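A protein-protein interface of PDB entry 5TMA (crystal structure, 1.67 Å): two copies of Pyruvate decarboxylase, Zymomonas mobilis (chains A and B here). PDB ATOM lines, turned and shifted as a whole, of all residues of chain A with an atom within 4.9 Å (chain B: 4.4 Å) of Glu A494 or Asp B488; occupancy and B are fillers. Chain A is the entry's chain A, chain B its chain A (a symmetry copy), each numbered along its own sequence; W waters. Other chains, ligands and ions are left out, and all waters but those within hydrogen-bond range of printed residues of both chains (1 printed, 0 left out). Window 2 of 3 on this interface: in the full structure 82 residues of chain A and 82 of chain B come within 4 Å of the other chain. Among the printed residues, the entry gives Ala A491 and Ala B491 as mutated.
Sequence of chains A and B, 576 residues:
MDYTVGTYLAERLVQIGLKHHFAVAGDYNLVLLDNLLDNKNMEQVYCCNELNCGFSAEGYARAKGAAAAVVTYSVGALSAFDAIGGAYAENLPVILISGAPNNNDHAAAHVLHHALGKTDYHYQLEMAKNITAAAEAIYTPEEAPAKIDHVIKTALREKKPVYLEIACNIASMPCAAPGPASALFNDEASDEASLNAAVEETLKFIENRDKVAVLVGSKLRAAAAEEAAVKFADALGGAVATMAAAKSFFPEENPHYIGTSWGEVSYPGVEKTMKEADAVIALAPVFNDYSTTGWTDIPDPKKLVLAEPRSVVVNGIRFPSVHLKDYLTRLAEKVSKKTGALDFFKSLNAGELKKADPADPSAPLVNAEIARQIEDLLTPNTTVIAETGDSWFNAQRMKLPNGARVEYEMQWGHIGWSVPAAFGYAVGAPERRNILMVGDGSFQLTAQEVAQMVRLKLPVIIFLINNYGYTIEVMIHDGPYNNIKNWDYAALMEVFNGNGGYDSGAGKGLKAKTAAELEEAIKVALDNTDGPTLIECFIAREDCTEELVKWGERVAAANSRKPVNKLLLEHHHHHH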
ATOM      1  N   ALA A 490     -12.010   7.401 -32.926  1.00  0.00           N
ATOM      2  CA  ALA A 490     -11.987   7.142 -31.485  1.00  0.00           C
ATOM      3  C   ALA A 490     -12.568   8.276 -30.670  1.00  0.00           C
ATOM      4  O   ALA A 490     -13.330   8.072 -29.731  1.00  0.00           O
ATOM      5  CB  ALA A 490     -10.562   6.840 -31.056  1.00  0.00           C
ATOM      6  N   ALA A 491     -12.294   9.509 -31.083  1.00  0.00           N
ATOM      7  CA  ALA A 491     -12.783  10.693 -30.371  1.00  0.00           C
ATOM      8  C   ALA A 491     -14.296  10.955 -30.481  1.00  0.00           C
ATOM      9  O   ALA A 491     -14.920  11.738 -29.683  1.00  0.00           O
ATOM     10  CB  ALA A 491     -11.996  11.941 -30.783  1.00  0.00           C
ATOM     11  N   LEU A 492     -14.897  10.290 -31.446  1.00  0.00           N
ATOM     12  CA  LEU A 492     -16.313  10.428 -31.673  1.00  0.00           C
ATOM     13  C   LEU A 492     -17.121   9.883 -30.519  1.00  0.00           C
ATOM     14  O   LEU A 492     -18.205  10.358 -30.249  1.00  0.00           O
ATOM     15  CB  LEU A 492     -16.625   9.812 -33.058  1.00  0.00           C
ATOM     16  CG  LEU A 492     -17.985   9.979 -33.635  1.00  0.00           C
ATOM     17  CD1 LEU A 492     -18.316  11.408 -33.864  1.00  0.00           C
ATOM     18  CD2 LEU A 492     -18.094   9.134 -34.914  1.00  0.00           C
ATOM     19  N   MET A 493     -16.571   8.917 -29.793  1.00  0.00           N
ATOM     20  CA  MET A 493     -17.248   8.350 -28.655  1.00  0.00           C
ATOM     21  C   MET A 493     -17.516   9.356 -27.542  1.00  0.00           C
ATOM     22  O   MET A 493     -18.628   9.378 -27.008  1.00  0.00           O
ATOM     23  CB  MET A 493     -16.570   7.093 -28.150  1.00  0.00           C
ATOM     24  CG  MET A 493     -16.405   6.069 -29.229  1.00  0.00           C
ATOM     25  SD  MET A 493     -17.947   5.545 -30.012  1.00  0.00           S
ATOM     26  CE  MET A 493     -18.497   4.567 -28.609  1.00  0.00           C
ATOM     27  N   GLU A 494     -16.558  10.255 -27.298  1.00  0.00           N
ATOM     28  CA  GLU A 494     -16.729  11.310 -26.330  1.00  0.00           C
ATOM     29  C   GLU A 494     -17.763  12.277 -26.776  1.00  0.00           C
ATOM     30  O   GLU A 494     -18.525  12.797 -25.970  1.00  0.00           O
ATOM     31  CB  GLU A 494     -15.409  12.079 -26.092  1.00  0.00           C
ATOM     32  CG  GLU A 494     -15.460  13.269 -25.133  1.00  0.00           C
ATOM     33  CD  GLU A 494     -16.029  14.651 -25.659  1.00  0.00           C
ATOM     34  OE1 GLU A 494     -15.952  14.995 -26.838  1.00  0.00           O
ATOM     35  OE2 GLU A 494     -16.647  15.414 -24.851  1.00  0.00           O
ATOM     36  N   VAL A 495     -17.834  12.514 -28.071  1.00  0.00           N
ATOM     37  CA  VAL A 495     -18.913  13.404 -28.613  1.00  0.00           C
ATOM     38  C   VAL A 495     -20.268  12.843 -28.249  1.00  0.00           C
ATOM     39  O   VAL A 495     -21.115  13.559 -27.774  1.00  0.00           O
ATOM     40  CB  VAL A 495     -18.804  13.556 -30.149  1.00  0.00           C
ATOM     41  CG1 VAL A 495     -20.022  14.281 -30.696  1.00  0.00           C
ATOM     42  CG2 VAL A 495     -17.484  14.275 -30.496  1.00  0.00           C
ATOM     43  N   PHE A 496     -20.460  11.531 -28.461  1.00  0.00           N
ATOM     44  CA  PHE A 496     -21.756  10.917 -28.215  1.00  0.00           C
ATOM     45  C   PHE A 496     -22.089  10.783 -26.733  1.00  0.00           C
ATOM     46  O   PHE A 496     -23.239  10.586 -26.362  1.00  0.00           O
ATOM     47  CB  PHE A 496     -21.817   9.581 -28.950  1.00  0.00           C
ATOM     48  CG  PHE A 496     -21.753   9.710 -30.457  1.00  0.00           C
ATOM     49  CD1 PHE A 496     -22.296  10.808 -31.137  1.00  0.00           C
ATOM     50  CD2 PHE A 496     -21.289   8.675 -31.240  1.00  0.00           C
ATOM     51  CE1 PHE A 496     -22.201  10.938 -32.515  1.00  0.00           C
ATOM     52  CE2 PHE A 496     -21.243   8.797 -32.623  1.00  0.00           C
ATOM     53  CZ  PHE A 496     -21.726   9.904 -33.270  1.00  0.00           C
ATOM     54  N   ASN A 497     -21.080  10.824 -25.884  1.00  0.00           N
ATOM     55  CA  ASN A 497     -21.323  10.803 -24.453  1.00  0.00           C
ATOM     56  C   ASN A 497     -21.935  12.048 -23.964  1.00  0.00           C
ATOM     57  O   ASN A 497     -22.663  11.952 -23.042  1.00  0.00           O
ATOM     58  CB  ASN A 497     -20.057  10.468 -23.673  1.00  0.00           C
ATOM     59  CG  ASN A 497     -19.725   9.037 -23.791  1.00  0.00           C
ATOM     60  OD1 ASN A 497     -20.587   8.207 -23.981  1.00  0.00           O
ATOM     61  ND2 ASN A 497     -18.511   8.718 -23.560  1.00  0.00           N
ATOM     62  N   GLY A 498     -21.737  13.188 -24.604  1.00  0.00           N
ATOM     63  CA  GLY A 498     -22.562  14.376 -24.309  1.00  0.00           C
ATOM     64  C   GLY A 498     -21.792  15.368 -23.457  1.00  0.00           C
ATOM     65  O   GLY A 498     -20.568  15.470 -23.608  1.00  0.00           O
ATOM     66  N   TRP B 487     -25.211  15.525 -27.588  1.00  0.00           N
ATOM     67  CA  TRP B 487     -23.824  15.376 -27.992  1.00  0.00           C
ATOM     68  C   TRP B 487     -22.992  16.551 -27.504  1.00  0.00           C
ATOM     69  O   TRP B 487     -23.554  17.655 -27.314  1.00  0.00           O
ATOM     70  CB  TRP B 487     -23.674  15.301 -29.522  1.00  0.00           C
ATOM     71  CG  TRP B 487     -24.418  14.197 -30.270  1.00  0.00           C
ATOM     72  CD1 TRP B 487     -25.141  13.139 -29.758  1.00  0.00           C
ATOM     73  CD2 TRP B 487     -24.424  14.037 -31.704  1.00  0.00           C
ATOM     74  NE1 TRP B 487     -25.591  12.360 -30.796  1.00  0.00           N
ATOM     75  CE2 TRP B 487     -25.161  12.905 -31.990  1.00  0.00           C
ATOM     76  CE3 TRP B 487     -23.865  14.782 -32.764  1.00  0.00           C
ATOM     77  CZ2 TRP B 487     -25.395  12.505 -33.301  1.00  0.00           C
ATOM     78  CZ3 TRP B 487     -24.085  14.396 -34.072  1.00  0.00           C
ATOM     79  CH2 TRP B 487     -24.807  13.243 -34.353  1.00  0.00           C
ATOM     80  N   ASP B 488     -21.670  16.360 -27.459  1.00  0.00           N
ATOM     81  CA  ASP B 488     -20.682  17.480 -27.406  1.00  0.00           C
ATOM     82  C   ASP B 488     -20.458  17.960 -28.831  1.00  0.00           C
ATOM     83  O   ASP B 488     -19.481  17.591 -29.487  1.00  0.00           O
ATOM     84  CB  ASP B 488     -19.386  17.023 -26.753  1.00  0.00           C
ATOM     85  CG  ASP B 488     -18.455  18.153 -26.440  1.00  0.00           C
ATOM     86  OD1 ASP B 488     -18.647  19.262 -27.009  1.00  0.00           O
ATOM     87  OD2 ASP B 488     -17.529  17.914 -25.638  1.00  0.00           O
ATOM     88  N   TYR B 489     -21.357  18.803 -29.286  1.00  0.00           N
ATOM     89  CA  TYR B 489     -21.311  19.241 -30.692  1.00  0.00           C
ATOM     90  C   TYR B 489     -20.014  19.940 -31.050  1.00  0.00           C
ATOM     91  O   TYR B 489     -19.429  19.736 -32.116  1.00  0.00           O
ATOM     92  CB  TYR B 489     -22.542  20.113 -31.021  1.00  0.00           C
ATOM     93  CG  TYR B 489     -23.846  19.391 -30.832  1.00  0.00           C
ATOM     94  CD1 TYR B 489     -24.351  18.582 -31.835  1.00  0.00           C
ATOM     95  CD2 TYR B 489     -24.592  19.508 -29.674  1.00  0.00           C
ATOM     96  CE1 TYR B 489     -25.527  17.880 -31.646  1.00  0.00           C
ATOM     97  CE2 TYR B 489     -25.774  18.787 -29.462  1.00  0.00           C
ATOM     98  CZ  TYR B 489     -26.237  17.979 -30.470  1.00  0.00           C
ATOM     99  OH  TYR B 489     -27.399  17.264 -30.301  1.00  0.00           O
ATOM    100  N   ALA B 490     -19.573  20.847 -30.170  1.00  0.00           N
ATOM    101  CA  ALA B 490     -18.319  21.572 -30.381  1.00  0.00           C
ATOM    102  C   ALA B 490     -17.139  20.657 -30.618  1.00  0.00           C
ATOM    103  O   ALA B 490     -16.311  20.885 -31.495  1.00  0.00           O
ATOM    104  CB  ALA B 490     -18.067  22.486 -29.196  1.00  0.00           C
ATOM    105  N   ALA B 491     -17.095  19.541 -29.900  1.00  0.00           N
ATOM    106  CA  ALA B 491     -15.996  18.579 -30.025  1.00  0.00           C
ATOM    107  C   ALA B 491     -15.962  17.777 -31.338  1.00  0.00           C
ATOM    108  O   ALA B 491     -14.921  17.146 -31.734  1.00  0.00           O
ATOM    109  CB  ALA B 491     -15.961  17.631 -28.822  1.00  0.00           C
ATOM    110  N   LEU B 492     -17.082  17.814 -32.031  1.00  0.00           N
ATOM    111  CA  LEU B 492     -17.205  17.114 -33.284  1.00  0.00           C
ATOM    112  C   LEU B 492     -16.296  17.695 -34.340  1.00  0.00           C
ATOM    113  O   LEU B 492     -15.843  16.990 -35.219  1.00  0.00           O
ATOM    114  CB  LEU B 492     -18.708  17.066 -33.646  1.00  0.00           C
ATOM    115  CG  LEU B 492     -19.149  16.243 -34.802  1.00  0.00           C
ATOM    116  CD1 LEU B 492     -18.847  14.803 -34.601  1.00  0.00           C
ATOM    117  CD2 LEU B 492     -20.641  16.502 -35.064  1.00  0.00           C
ATOM    118  N   LYS B 511     -17.976  26.901 -27.848  1.00  0.00           N
ATOM    119  CA  LYS B 511     -19.130  26.817 -27.015  1.00  0.00           C
ATOM    120  C   LYS B 511     -19.523  28.245 -26.616  1.00  0.00           C
ATOM    121  O   LYS B 511     -18.678  29.049 -26.260  1.00  0.00           O
ATOM    122  CB  LYS B 511     -18.842  25.919 -25.805  1.00  0.00           C
ATOM    123  CG  LYS B 511     -18.901  24.448 -26.102  1.00  0.00           C
ATOM    124  CD  LYS B 511     -18.458  23.560 -24.941  1.00  0.00           C
ATOM    125  CE  LYS B 511     -18.336  22.072 -25.294  1.00  0.00           C
ATOM    126  NZ  LYS B 511     -19.646  21.374 -25.681  1.00  0.00           N
ATOM    127  N   GLU B 536     -21.592  26.256 -30.690  1.00  0.00           N
ATOM    128  CA  GLU B 536     -22.595  25.520 -30.010  1.00  0.00           C
ATOM    129  C   GLU B 536     -23.211  26.468 -28.999  1.00  0.00           C
ATOM    130  O   GLU B 536     -22.538  26.815 -28.010  1.00  0.00           O
ATOM    131  CB  GLU B 536     -22.034  24.268 -29.355  1.00  0.00           C
ATOM    132  CG  GLU B 536     -23.047  23.433 -28.632  1.00  0.00           C
ATOM    133  CD  GLU B 536     -22.547  22.199 -27.923  1.00  0.00           C
ATOM    134  OE1 GLU B 536     -21.341  21.916 -27.891  1.00  0.00           O
ATOM    135  OE2 GLU B 536     -23.390  21.575 -27.310  1.00  0.00           O
HETATM  136  O   HOH W   1     -19.149  18.285 -22.998  1.00  0.00           O
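Water W1 lies within hydrogen-bond range of the side-chain carboxylate of Asp B488 (3.1 Å) and the backbone carbonyl oxygen of Gly A498 (3.2 Å).
Printed residues of chain B that touch a printed residue of chain A: Trp B487, Asp B488, Ala B491 and Leu B492. Among the printed residues, no Asp or Glu carboxylate lies within 4 Å of a Lys or Arg side-chain nitrogen of the other chain.
CD1 of Leu A492 touches CD1 of Leu B492, 3.5 Å away. OE1 of Glu A494 touches CB of Ala B491, at 3.3 Å. Val A495 touches Trp B487. C of Ala B491 touches CG2 of Val A495 (3.9 Å). N of Leu B492 touches CG2 of Val A495 (3.9 Å). Phe A496 touches Trp B487. Gly A498 touches Trp B487. CB of Asp B488 touches O of Gly A498, 3.7 Å away.
The backbone carbonyl oxygen of Val A495 lies within hydrogen-bond range of the backbone NH of Asp B488, 2.9 Å away. The side-chain carboxylate (OE2) of Glu A494 sits close to the side-chain carboxylate (OD2) of Asp B488, 2.8 Å away.
Leu A492 touches its own counterpart, Leu B492.
Glu A494 touches two residues of chain B. Of chain A, only Glu A494 (2.8 Å), Val A495 (2.9 Å) and Gly A498 (3.7 Å) come within 4 Å of Asp B488. Of the printed residues of chain A, Leu B492 touches Leu A492 and Val A495. Printed residues of chain B within 4 Å of Leu A492: Leu B492. Glu B536 touches none of the printed residues of chain A. Tyr B489 touches none of the printed residues of chain A. The nearest printed residue of chain B that does not touch Gly A498 is Lys B511 (6.3 Å).
OD1 of Asp B488 sits at hydrogen-bond distance from N of Ala B491. The side-chain amino group of Lys B511 lies within salt-bridge range of the side-chain carboxylate of Asp B488.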
